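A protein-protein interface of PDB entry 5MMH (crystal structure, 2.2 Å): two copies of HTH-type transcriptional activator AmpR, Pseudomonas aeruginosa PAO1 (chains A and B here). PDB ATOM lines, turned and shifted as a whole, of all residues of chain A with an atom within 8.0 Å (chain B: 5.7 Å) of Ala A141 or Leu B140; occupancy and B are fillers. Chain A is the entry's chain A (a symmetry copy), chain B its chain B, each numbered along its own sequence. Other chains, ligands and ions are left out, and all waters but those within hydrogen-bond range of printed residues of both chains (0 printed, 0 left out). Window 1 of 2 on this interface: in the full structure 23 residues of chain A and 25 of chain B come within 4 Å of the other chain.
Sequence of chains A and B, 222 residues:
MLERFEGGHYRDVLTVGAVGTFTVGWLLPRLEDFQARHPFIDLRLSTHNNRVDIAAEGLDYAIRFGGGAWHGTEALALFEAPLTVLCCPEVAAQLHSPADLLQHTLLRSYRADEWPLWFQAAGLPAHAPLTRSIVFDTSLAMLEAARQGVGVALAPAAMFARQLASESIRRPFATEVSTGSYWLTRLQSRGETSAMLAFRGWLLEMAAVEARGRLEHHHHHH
N of Thr B47 sits at hydrogen-bond distance from O of Val A135 (3.1 Å). O of Val B24 lies close to OE1 of Gln A148 (3.3 Å). The side-chain hydroxyl of Thr B47 is in hydrogen-bond range of the side-chain carboxylate of Asp A137 (2.7 Å).
The backbone NH (N) of Leu B140 lies within hydrogen-bond range of the side-chain hydroxyl (OG1) of Thr B21, at 3.4 Å. OG1 of Thr A138 sits close to N of Leu A140. The side-chain hydroxyl (OG1) of Thr B138 sits at hydrogen-bond distance from the backbone NH (N) of Ala B141, at 3.3 Å. NE2 of Gln A148 sits at hydrogen-bond distance from OE1 of Glu A144 (2.5 Å). O of Ala A145 lies within hydrogen-bond range of N of Val A150, at 3.1 Å.
Among the printed residues, merely in contact across the chains: Val A24 with Ala B141, Val A24 with Glu B144, Phe A136 with Thr B47, Leu A140 with Ala B141, Ala A141 with Val B24, Ala A141 with Leu B140, Glu A144 with Val B24 and Ala A145 with Val B24.
Of the printed residues of chain B, Leu A140 touches Ala B141 (3.9 Å). Ala A141 touches two residues of chain B. Printed residues of chain B within 4 Å of Glu A144: Val B24 (3.5 Å). Of the printed residues of chain B, Ala A145 touches Val B24 (3.5 Å). Phe A160 touches none of the printed residues of chain B. Thr B21 touches none of the printed residues of chain A. Of the printed residues of chain A, Thr B47 touches Val A135, Phe A136 and Asp A137. Leu B140 touches just one residue of chain A: Ala A141 (3.6 Å). Of the printed residues of chain A, Glu B144 touches Val A24. The nearest residue of chain A that does not touch Leu B140 is Leu A140 (4.4 Å). The nearest printed residue of chain B that does not touch Gln A148 is Leu B140 (7.7 Å).
Printed residues of chain A that touch a printed residue of chain B: Val A24, Val A135, Phe A136, Asp A137, Leu A140, Ala A141, Glu A144, Ala A145 and Gln A148. Hydrophobic or aromatic side chains of chain A within 4 Å of the printed part of chain B: Val A24, Leu A140 and Ala A141. Among the printed residues, no Asp or Glu carboxylate lies within 4 Å of a Lys or Arg side-chain nitrogen of the other chain.
Val A24 touches Ala B141, and with the chains exchanged Ala A141 touches Val B24. Val A24 touches Glu B144, and with the chains exchanged Glu A144 touches Val B24. Leu A140 touches Ala B141, and with the chains exchanged Ala A141 touches Leu B140. Ala A145 touches Val B24, but with the chains exchanged Val A24 does not touch Ala B145 (4.2 Å).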
ATOM      1  N   GLY A  20     -12.803 -16.369 -23.076  1.00  0.00           N
ATOM      2  CA  GLY A  20     -13.273 -17.489 -22.279  1.00  0.00           C
ATOM      3  C   GLY A  20     -14.743 -17.398 -21.935  1.00  0.00           C
ATOM      4  O   GLY A  20     -15.480 -18.384 -22.041  1.00  0.00           O
ATOM      5  N   THR A  21     -15.197 -16.207 -21.561  1.00  0.00           N
ATOM      6  CA  THR A  21     -16.604 -16.003 -21.218  1.00  0.00           C
ATOM      7  C   THR A  21     -17.524 -16.384 -22.371  1.00  0.00           C
ATOM      8  O   THR A  21     -18.568 -17.018 -22.160  1.00  0.00           O
ATOM      9  CB  THR A  21     -16.825 -14.541 -20.815  1.00  0.00           C
ATOM     10  OG1 THR A  21     -16.017 -14.255 -19.662  1.00  0.00           O
ATOM     11  CG2 THR A  21     -18.318 -14.247 -20.503  1.00  0.00           C
ATOM     12  N   VAL A  24     -17.427 -20.574 -22.928  1.00  0.00           N
ATOM     13  CA  VAL A  24     -18.170 -21.470 -22.044  1.00  0.00           C
ATOM     14  C   VAL A  24     -19.615 -21.021 -21.900  1.00  0.00           C
ATOM     15  O   VAL A  24     -20.499 -21.861 -21.760  1.00  0.00           O
ATOM     16  CB  VAL A  24     -17.502 -21.635 -20.659  1.00  0.00           C
ATOM     17  CG1 VAL A  24     -16.106 -22.179 -20.813  1.00  0.00           C
ATOM     18  CG2 VAL A  24     -17.454 -20.342 -19.911  1.00  0.00           C
ATOM     19  N   THR A  47      -9.044 -20.727 -25.625  1.00  0.00           N
ATOM     20  CA  THR A  47      -9.643 -19.536 -25.046  1.00  0.00           C
ATOM     21  C   THR A  47      -8.556 -18.528 -24.707  1.00  0.00           C
ATOM     22  O   THR A  47      -7.382 -18.869 -24.571  1.00  0.00           O
ATOM     23  CB  THR A  47     -10.487 -19.827 -23.791  1.00  0.00           C
ATOM     24  OG1 THR A  47      -9.655 -20.264 -22.687  1.00  0.00           O
ATOM     25  CG2 THR A  47     -11.572 -20.856 -24.100  1.00  0.00           C
ATOM     26  N   LEU A 107     -17.447  -4.916  -8.391  1.00  0.00           N
ATOM     27  CA  LEU A 107     -16.502  -5.685  -9.192  1.00  0.00           C
ATOM     28  C   LEU A 107     -16.478  -5.130 -10.610  1.00  0.00           C
ATOM     29  O   LEU A 107     -17.527  -4.859 -11.196  1.00  0.00           O
ATOM     30  CB  LEU A 107     -16.906  -7.155  -9.204  1.00  0.00           C
ATOM     31  CG  LEU A 107     -17.254  -7.780  -7.850  1.00  0.00           C
ATOM     32  CD1 LEU A 107     -17.911  -9.122  -8.062  1.00  0.00           C
ATOM     33  CD2 LEU A 107     -15.982  -7.918  -6.929  1.00  0.00           C
ATOM     34  N   VAL A 135     -10.471  -5.422  -9.897  1.00  0.00           N
ATOM     35  CA  VAL A 135     -10.481  -5.410 -11.358  1.00  0.00           C
ATOM     36  C   VAL A 135     -10.226  -6.823 -11.859  1.00  0.00           C
ATOM     37  O   VAL A 135      -9.324  -7.514 -11.365  1.00  0.00           O
ATOM     38  CB  VAL A 135      -9.426  -4.431 -11.917  1.00  0.00           C
ATOM     39  CG1 VAL A 135      -9.488  -4.395 -13.437  1.00  0.00           C
ATOM     40  CG2 VAL A 135      -9.616  -3.047 -11.328  1.00  0.00           C
ATOM     41  N   PHE A 136     -10.995  -7.246 -12.859  1.00  0.00           N
ATOM     42  CA  PHE A 136     -11.003  -8.632 -13.305  1.00  0.00           C
ATOM     43  C   PHE A 136     -10.632  -8.722 -14.776  1.00  0.00           C
ATOM     44  O   PHE A 136     -11.115  -7.934 -15.590  1.00  0.00           O
ATOM     45  CB  PHE A 136     -12.377  -9.270 -13.070  1.00  0.00           C
ATOM     46  CG  PHE A 136     -12.643  -9.607 -11.637  1.00  0.00           C
ATOM     47  CD1 PHE A 136     -13.297  -8.708 -10.805  1.00  0.00           C
ATOM     48  CD2 PHE A 136     -12.214 -10.814 -11.110  1.00  0.00           C
ATOM     49  CE1 PHE A 136     -13.533  -9.017  -9.474  1.00  0.00           C
ATOM     50  CE2 PHE A 136     -12.438 -11.129  -9.787  1.00  0.00           C
ATOM     51  CZ  PHE A 136     -13.105 -10.233  -8.965  1.00  0.00           C
ATOM     52  N   ASP A 137      -9.772  -9.684 -15.106  1.00  0.00           N
ATOM     53  CA  ASP A 137      -9.376  -9.883 -16.490  1.00  0.00           C
ATOM     54  C   ASP A 137     -10.463 -10.591 -17.278  1.00  0.00           C
ATOM     55  O   ASP A 137     -10.524 -10.440 -18.497  1.00  0.00           O
ATOM     56  CB  ASP A 137      -8.052 -10.665 -16.575  1.00  0.00           C
ATOM     57  CG  ASP A 137      -8.199 -12.202 -16.273  1.00  0.00           C
ATOM     58  OD1 ASP A 137      -8.790 -12.596 -15.223  1.00  0.00           O
ATOM     59  OD2 ASP A 137      -7.647 -13.028 -17.066  1.00  0.00           O
ATOM     60  N   THR A 138     -11.328 -11.342 -16.606  1.00  0.00           N
ATOM     61  CA  THR A 138     -12.347 -12.159 -17.252  1.00  0.00           C
ATOM     62  C   THR A 138     -13.616 -12.097 -16.417  1.00  0.00           C
ATOM     63  O   THR A 138     -13.558 -12.134 -15.180  1.00  0.00           O
ATOM     64  CB  THR A 138     -11.879 -13.641 -17.431  1.00  0.00           C
ATOM     65  OG1 THR A 138     -12.968 -14.469 -17.853  1.00  0.00           O
ATOM     66  CG2 THR A 138     -11.370 -14.204 -16.171  1.00  0.00           C
ATOM     67  N   SER A 139     -14.755 -12.001 -17.106  1.00  0.00           N
ATOM     68  CA  SER A 139     -16.045 -11.988 -16.430  1.00  0.00           C
ATOM     69  C   SER A 139     -16.295 -13.285 -15.688  1.00  0.00           C
ATOM     70  O   SER A 139     -17.009 -13.293 -14.677  1.00  0.00           O
ATOM     71  CB  SER A 139     -17.171 -11.750 -17.445  1.00  0.00           C
ATOM     72  OG  SER A 139     -17.067 -10.462 -18.023  1.00  0.00           O
ATOM     73  N   LEU A 140     -15.739 -14.394 -16.176  1.00  0.00           N
ATOM     74  CA  LEU A 140     -15.855 -15.647 -15.434  1.00  0.00           C
ATOM     75  C   LEU A 140     -15.308 -15.493 -14.024  1.00  0.00           C
ATOM     76  O   LEU A 140     -15.940 -15.925 -13.054  1.00  0.00           O
ATOM     77  CB  LEU A 140     -15.120 -16.763 -16.161  1.00  0.00           C
ATOM     78  CG  LEU A 140     -15.781 -17.237 -17.453  1.00  0.00           C
ATOM     79  CD1 LEU A 140     -14.863 -18.258 -18.093  1.00  0.00           C
ATOM     80  CD2 LEU A 140     -17.177 -17.813 -17.203  1.00  0.00           C
ATOM     81  N   ALA A 141     -14.132 -14.874 -13.887  1.00  0.00           N
ATOM     82  CA  ALA A 141     -13.580 -14.683 -12.552  1.00  0.00           C
ATOM     83  C   ALA A 141     -14.435 -13.706 -11.761  1.00  0.00           C
ATOM     84  O   ALA A 141     -14.643 -13.895 -10.557  1.00  0.00           O
ATOM     85  CB  ALA A 141     -12.133 -14.188 -12.636  1.00  0.00           C
ATOM     86  N   MET A 142     -14.964 -12.676 -12.440  1.00  0.00           N
ATOM     87  CA  MET A 142     -15.825 -11.686 -11.799  1.00  0.00           C
ATOM     88  C   MET A 142     -17.137 -12.298 -11.312  1.00  0.00           C
ATOM     89  O   MET A 142     -17.640 -11.920 -10.245  1.00  0.00           O
ATOM     90  CB  MET A 142     -16.108 -10.542 -12.772  1.00  0.00           C
ATOM     91  CG  MET A 142     -17.034  -9.481 -12.212  1.00  0.00           C
ATOM     92  SD  MET A 142     -17.800  -8.391 -13.450  1.00  0.00           S
ATOM     93  CE  MET A 142     -16.371  -7.598 -14.196  1.00  0.00           C
ATOM     94  N   LEU A 143     -17.708 -13.246 -12.070  1.00  0.00           N
ATOM     95  CA  LEU A 143     -18.994 -13.819 -11.671  1.00  0.00           C
ATOM     96  C   LEU A 143     -18.831 -14.845 -10.562  1.00  0.00           C
ATOM     97  O   LEU A 143     -19.692 -14.954  -9.681  1.00  0.00           O
ATOM     98  CB  LEU A 143     -19.696 -14.448 -12.872  1.00  0.00           C
ATOM     99  CG  LEU A 143     -20.782 -13.543 -13.462  1.00  0.00           C
ATOM    100  CD1 LEU A 143     -21.870 -13.285 -12.433  1.00  0.00           C
ATOM    101  CD2 LEU A 143     -20.194 -12.221 -13.952  1.00  0.00           C
ATOM    102  N   GLU A 144     -17.745 -15.620 -10.609  1.00  0.00           N
ATOM    103  CA  GLU A 144     -17.393 -16.487  -9.492  1.00  0.00           C
ATOM    104  C   GLU A 144     -17.180 -15.681  -8.207  1.00  0.00           C
ATOM    105  O   GLU A 144     -17.650 -16.081  -7.136  1.00  0.00           O
ATOM    106  CB  GLU A 144     -16.148 -17.304  -9.844  1.00  0.00           C
ATOM    107  CG  GLU A 144     -15.659 -18.200  -8.715  1.00  0.00           C
ATOM    108  CD  GLU A 144     -16.609 -19.341  -8.397  1.00  0.00           C
ATOM    109  OE1 GLU A 144     -16.553 -19.864  -7.256  1.00  0.00           O
ATOM    110  OE2 GLU A 144     -17.390 -19.736  -9.295  1.00  0.00           O
ATOM    111  N   ALA A 145     -16.498 -14.531  -8.291  1.00  0.00           N
ATOM    112  CA  ALA A 145     -16.373 -13.680  -7.108  1.00  0.00           C
ATOM    113  C   ALA A 145     -17.733 -13.203  -6.627  1.00  0.00           C
ATOM    114  O   ALA A 145     -17.992 -13.152  -5.420  1.00  0.00           O
ATOM    115  CB  ALA A 145     -15.476 -12.478  -7.396  1.00  0.00           C
ATOM    116  N   ALA A 146     -18.620 -12.850  -7.560  1.00  0.00           N
ATOM    117  CA  ALA A 146     -19.950 -12.397  -7.178  1.00  0.00           C
ATOM    118  C   ALA A 146     -20.753 -13.529  -6.563  1.00  0.00           C
ATOM    119  O   ALA A 146     -21.471 -13.322  -5.584  1.00  0.00           O
ATOM    120  CB  ALA A 146     -20.682 -11.827  -8.393  1.00  0.00           C
ATOM    121  N   ARG A 147     -20.654 -14.729  -7.134  1.00  0.00           N
ATOM    122  CA  ARG A 147     -21.280 -15.902  -6.527  1.00  0.00           C
ATOM    123  C   ARG A 147     -20.918 -16.030  -5.048  1.00  0.00           C
ATOM    124  O   ARG A 147     -21.788 -16.250  -4.196  1.00  0.00           O
ATOM    125  CB  ARG A 147     -20.857 -17.168  -7.279  1.00  0.00           C
ATOM    126  CG  ARG A 147     -21.667 -18.418  -6.906  1.00  0.00           C
ATOM    127  CD  ARG A 147     -22.526 -18.821  -8.032  1.00  0.00           C
ATOM    128  NE  ARG A 147     -21.804 -19.625  -9.017  1.00  0.00           N
ATOM    129  CZ  ARG A 147     -22.352 -20.219 -10.076  1.00  0.00           C
ATOM    130  NH1 ARG A 147     -21.588 -20.923 -10.883  1.00  0.00           N
ATOM    131  NH2 ARG A 147     -23.642 -20.051 -10.343  1.00  0.00           N
ATOM    132  N   GLN A 148     -19.626 -15.916  -4.733  1.00  0.00           N
ATOM    133  CA  GLN A 148     -19.121 -16.076  -3.375  1.00  0.00           C
ATOM    134  C   GLN A 148     -19.367 -14.856  -2.492  1.00  0.00           C
ATOM    135  O   GLN A 148     -18.796 -14.777  -1.400  1.00  0.00           O
ATOM    136  CB  GLN A 148     -17.623 -16.404  -3.417  1.00  0.00           C
ATOM    137  CG  GLN A 148     -17.331 -17.869  -3.724  1.00  0.00           C
ATOM    138  CD  GLN A 148     -15.868 -18.129  -4.055  1.00  0.00           C
ATOM    139  OE1 GLN A 148     -14.962 -17.664  -3.354  1.00  0.00           O
ATOM    140  NE2 GLN A 148     -15.631 -18.892  -5.115  1.00  0.00           N
ATOM    141  N   VAL A 150     -18.490 -11.686  -2.748  1.00  0.00           N
ATOM    142  CA  VAL A 150     -17.458 -10.668  -2.613  1.00  0.00           C
ATOM    143  C   VAL A 150     -17.967  -9.289  -3.027  1.00  0.00           C
ATOM    144  O   VAL A 150     -17.571  -8.272  -2.442  1.00  0.00           O
ATOM    145  CB  VAL A 150     -16.232 -11.105  -3.428  1.00  0.00           C
ATOM    146  CG1 VAL A 150     -15.151 -10.087  -3.349  1.00  0.00           C
ATOM    147  CG2 VAL A 150     -15.735 -12.484  -2.918  1.00  0.00           C
ATOM    148  N   ALA A 153     -21.358  -7.672  -9.548  1.00  0.00           N
ATOM    149  CA  ALA A 153     -20.781  -7.758 -10.885  1.00  0.00           C
ATOM    150  C   ALA A 153     -21.546  -6.920 -11.907  1.00  0.00           C
ATOM    151  O   ALA A 153     -22.747  -6.670 -11.777  1.00  0.00           O
ATOM    152  CB  ALA A 153     -20.738  -9.206 -11.364  1.00  0.00           C
ATOM    153  N   PHE A 160     -24.304 -15.544 -19.071  1.00  0.00           N
ATOM    154  CA  PHE A 160     -24.490 -16.275 -17.820  1.00  0.00           C
ATOM    155  C   PHE A 160     -25.937 -16.713 -17.688  1.00  0.00           C
ATOM    156  O   PHE A 160     -26.542 -16.652 -16.616  1.00  0.00           O
ATOM    157  CB  PHE A 160     -24.026 -15.431 -16.639  1.00  0.00           C
ATOM    158  CG  PHE A 160     -22.576 -15.100 -16.709  1.00  0.00           C
ATOM    159  CD1 PHE A 160     -21.623 -16.011 -16.270  1.00  0.00           C
ATOM    160  CD2 PHE A 160     -22.155 -13.912 -17.270  1.00  0.00           C
ATOM    161  CE1 PHE A 160     -20.283 -15.719 -16.378  1.00  0.00           C
ATOM    162  CE2 PHE A 160     -20.808 -13.614 -17.372  1.00  0.00           C
ATOM    163  CZ  PHE A 160     -19.880 -14.510 -16.942  1.00  0.00           C
ATOM    164  N   GLY B  20      -6.032 -15.483 -11.966  1.00  0.00           N
ATOM    165  CA  GLY B  20      -7.440 -15.366 -11.611  1.00  0.00           C
ATOM    166  C   GLY B  20      -7.984 -16.571 -10.873  1.00  0.00           C
ATOM    167  O   GLY B  20      -8.738 -16.434  -9.902  1.00  0.00           O
ATOM    168  N   THR B  21      -7.597 -17.759 -11.311  1.00  0.00           N
ATOM    169  CA  THR B  21      -7.955 -18.987 -10.615  1.00  0.00           C
ATOM    170  C   THR B  21      -7.576 -18.940  -9.135  1.00  0.00           C
ATOM    171  O   THR B  21      -8.380 -19.316  -8.267  1.00  0.00           O
ATOM    172  CB  THR B  21      -7.278 -20.160 -11.321  1.00  0.00           C
ATOM    173  OG1 THR B  21      -7.880 -20.340 -12.625  1.00  0.00           O
ATOM    174  CG2 THR B  21      -7.412 -21.433 -10.501  1.00  0.00           C
ATOM    175  N   VAL B  24      -9.824 -16.207  -7.022  1.00  0.00           N
ATOM    176  CA  VAL B  24     -11.201 -16.525  -6.730  1.00  0.00           C
ATOM    177  C   VAL B  24     -11.321 -17.837  -5.960  1.00  0.00           C
ATOM    178  O   VAL B  24     -12.224 -17.997  -5.135  1.00  0.00           O
ATOM    179  CB  VAL B  24     -11.963 -16.539  -8.074  1.00  0.00           C
ATOM    180  CG1 VAL B  24     -12.196 -17.949  -8.591  1.00  0.00           C
ATOM    181  CG2 VAL B  24     -13.230 -15.748  -7.974  1.00  0.00           C
ATOM    182  N   THR B  47      -6.659  -9.152 -11.503  1.00  0.00           N
ATOM    183  CA  THR B  47      -6.345 -10.518 -11.911  1.00  0.00           C
ATOM    184  C   THR B  47      -5.744 -10.536 -13.310  1.00  0.00           C
ATOM    185  O   THR B  47      -5.821  -9.565 -14.059  1.00  0.00           O
ATOM    186  CB  THR B  47      -7.562 -11.474 -11.855  1.00  0.00           C
ATOM    187  OG1 THR B  47      -8.529 -11.192 -12.891  1.00  0.00           O
ATOM    188  CG2 THR B  47      -8.229 -11.417 -10.495  1.00  0.00           C
ATOM    189  N   THR B 138      -7.284 -20.185 -18.750  1.00  0.00           N
ATOM    190  CA  THR B 138      -7.485 -20.163 -17.308  1.00  0.00           C
ATOM    191  C   THR B 138      -8.121 -21.479 -16.899  1.00  0.00           C
ATOM    192  O   THR B 138      -8.947 -22.026 -17.636  1.00  0.00           O
ATOM    193  CB  THR B 138      -8.400 -18.991 -16.860  1.00  0.00           C
ATOM    194  OG1 THR B 138      -9.658 -19.064 -17.547  1.00  0.00           O
ATOM    195  CG2 THR B 138      -7.764 -17.649 -17.168  1.00  0.00           C
ATOM    196  N   SER B 139      -7.746 -21.986 -15.726  1.00  0.00           N
ATOM    197  CA  SER B 139      -8.463 -23.139 -15.186  1.00  0.00           C
ATOM    198  C   SER B 139      -9.919 -22.821 -14.916  1.00  0.00           C
ATOM    199  O   SER B 139     -10.747 -23.735 -14.848  1.00  0.00           O
ATOM    200  CB  SER B 139      -7.818 -23.640 -13.890  1.00  0.00           C
ATOM    201  OG  SER B 139      -6.536 -24.173 -14.145  1.00  0.00           O
ATOM    202  N   LEU B 140     -10.251 -21.548 -14.712  1.00  0.00           N
ATOM    203  CA  LEU B 140     -11.651 -21.197 -14.498  1.00  0.00           C
ATOM    204  C   LEU B 140     -12.494 -21.586 -15.707  1.00  0.00           C
ATOM    205  O   LEU B 140     -13.534 -22.248 -15.569  1.00  0.00           O
ATOM    206  CB  LEU B 140     -11.788 -19.704 -14.211  1.00  0.00           C
ATOM    207  CG  LEU B 140     -11.301 -19.206 -12.863  1.00  0.00           C
ATOM    208  CD1 LEU B 140     -11.722 -17.754 -12.774  1.00  0.00           C
ATOM    209  CD2 LEU B 140     -11.903 -20.024 -11.721  1.00  0.00           C
ATOM    210  N   ALA B 141     -12.062 -21.174 -16.907  1.00  0.00           N
ATOM    211  CA  ALA B 141     -12.794 -21.560 -18.107  1.00  0.00           C
ATOM    212  C   ALA B 141     -12.814 -23.076 -18.258  1.00  0.00           C
ATOM    213  O   ALA B 141     -13.851 -23.661 -18.579  1.00  0.00           O
ATOM    214  CB  ALA B 141     -12.174 -20.899 -19.340  1.00  0.00           C
ATOM    215  N   MET B 142     -11.679 -23.730 -17.998  1.00  0.00           N
ATOM    216  CA  MET B 142     -11.604 -25.185 -18.088  1.00  0.00           C
ATOM    217  C   MET B 142     -12.595 -25.877 -17.157  1.00  0.00           C
ATOM    218  O   MET B 142     -13.219 -26.875 -17.530  1.00  0.00           O
ATOM    219  CB  MET B 142     -10.187 -25.648 -17.756  1.00  0.00           C
ATOM    220  CG  MET B 142      -9.951 -27.100 -18.046  1.00  0.00           C
ATOM    221  SD  MET B 142      -8.494 -27.724 -17.201  1.00  0.00           S
ATOM    222  CE  MET B 142      -7.161 -26.998 -18.125  1.00  0.00           C
ATOM    223  N   LEU B 143     -12.722 -25.402 -15.925  1.00  0.00           N
ATOM    224  CA  LEU B 143     -13.602 -26.094 -14.989  1.00  0.00           C
ATOM    225  C   LEU B 143     -15.073 -25.898 -15.337  1.00  0.00           C
ATOM    226  O   LEU B 143     -15.884 -26.794 -15.088  1.00  0.00           O
ATOM    227  CB  LEU B 143     -13.310 -25.641 -13.562  1.00  0.00           C
ATOM    228  CG  LEU B 143     -12.546 -26.749 -12.823  1.00  0.00           C
ATOM    229  CD1 LEU B 143     -13.462 -27.977 -12.689  1.00  0.00           C
ATOM    230  CD2 LEU B 143     -11.273 -27.107 -13.593  1.00  0.00           C
ATOM    231  N   GLU B 144     -15.433 -24.750 -15.923  1.00  0.00           N
ATOM    232  CA  GLU B 144     -16.809 -24.535 -16.352  1.00  0.00           C
ATOM    233  C   GLU B 144     -17.167 -25.410 -17.544  1.00  0.00           C
ATOM    234  O   GLU B 144     -18.312 -25.859 -17.659  1.00  0.00           O
ATOM    235  CB  GLU B 144     -17.037 -23.061 -16.683  1.00  0.00           C
ATOM    236  CG  GLU B 144     -18.416 -22.740 -17.199  1.00  0.00           C
ATOM    237  CD  GLU B 144     -19.529 -23.148 -16.241  1.00  0.00           C
ATOM    238  OE1 GLU B 144     -19.305 -23.103 -15.005  1.00  0.00           O
ATOM    239  OE2 GLU B 144     -20.635 -23.495 -16.732  1.00  0.00           O
ATOM    240  N   ALA B 145     -16.213 -25.682 -18.435  1.00  0.00           N
ATOM    241  CA  ALA B 145     -16.517 -26.622 -19.513  1.00  0.00           C
ATOM    242  C   ALA B 145     -16.668 -28.033 -18.968  1.00  0.00           C
ATOM    243  O   ALA B 145     -17.445 -28.828 -19.505  1.00  0.00           O
ATOM    244  CB  ALA B 145     -15.430 -26.576 -20.594  1.00  0.00           C
ATOM    245  N   PHE B 160     -10.603 -25.424  -6.321  1.00  0.00           N
ATOM    246  CA  PHE B 160     -12.011 -25.648  -6.630  1.00  0.00           C
ATOM    247  C   PHE B 160     -12.694 -26.394  -5.496  1.00  0.00           C
ATOM    248  O   PHE B 160     -13.515 -27.297  -5.709  1.00  0.00           O
ATOM    249  CB  PHE B 160     -12.159 -26.383  -7.960  1.00  0.00           C
ATOM    250  CG  PHE B 160     -11.542 -25.635  -9.113  1.00  0.00           C
ATOM    251  CD1 PHE B 160     -12.283 -24.703  -9.830  1.00  0.00           C
ATOM    252  CD2 PHE B 160     -10.206 -25.826  -9.441  1.00  0.00           C
ATOM    253  CE1 PHE B 160     -11.701 -23.994 -10.861  1.00  0.00           C
ATOM    254  CE2 PHE B 160      -9.614 -25.125 -10.475  1.00  0.00           C
ATOM    255  CZ  PHE B 160     -10.369 -24.204 -11.197  1.00  0.00           C
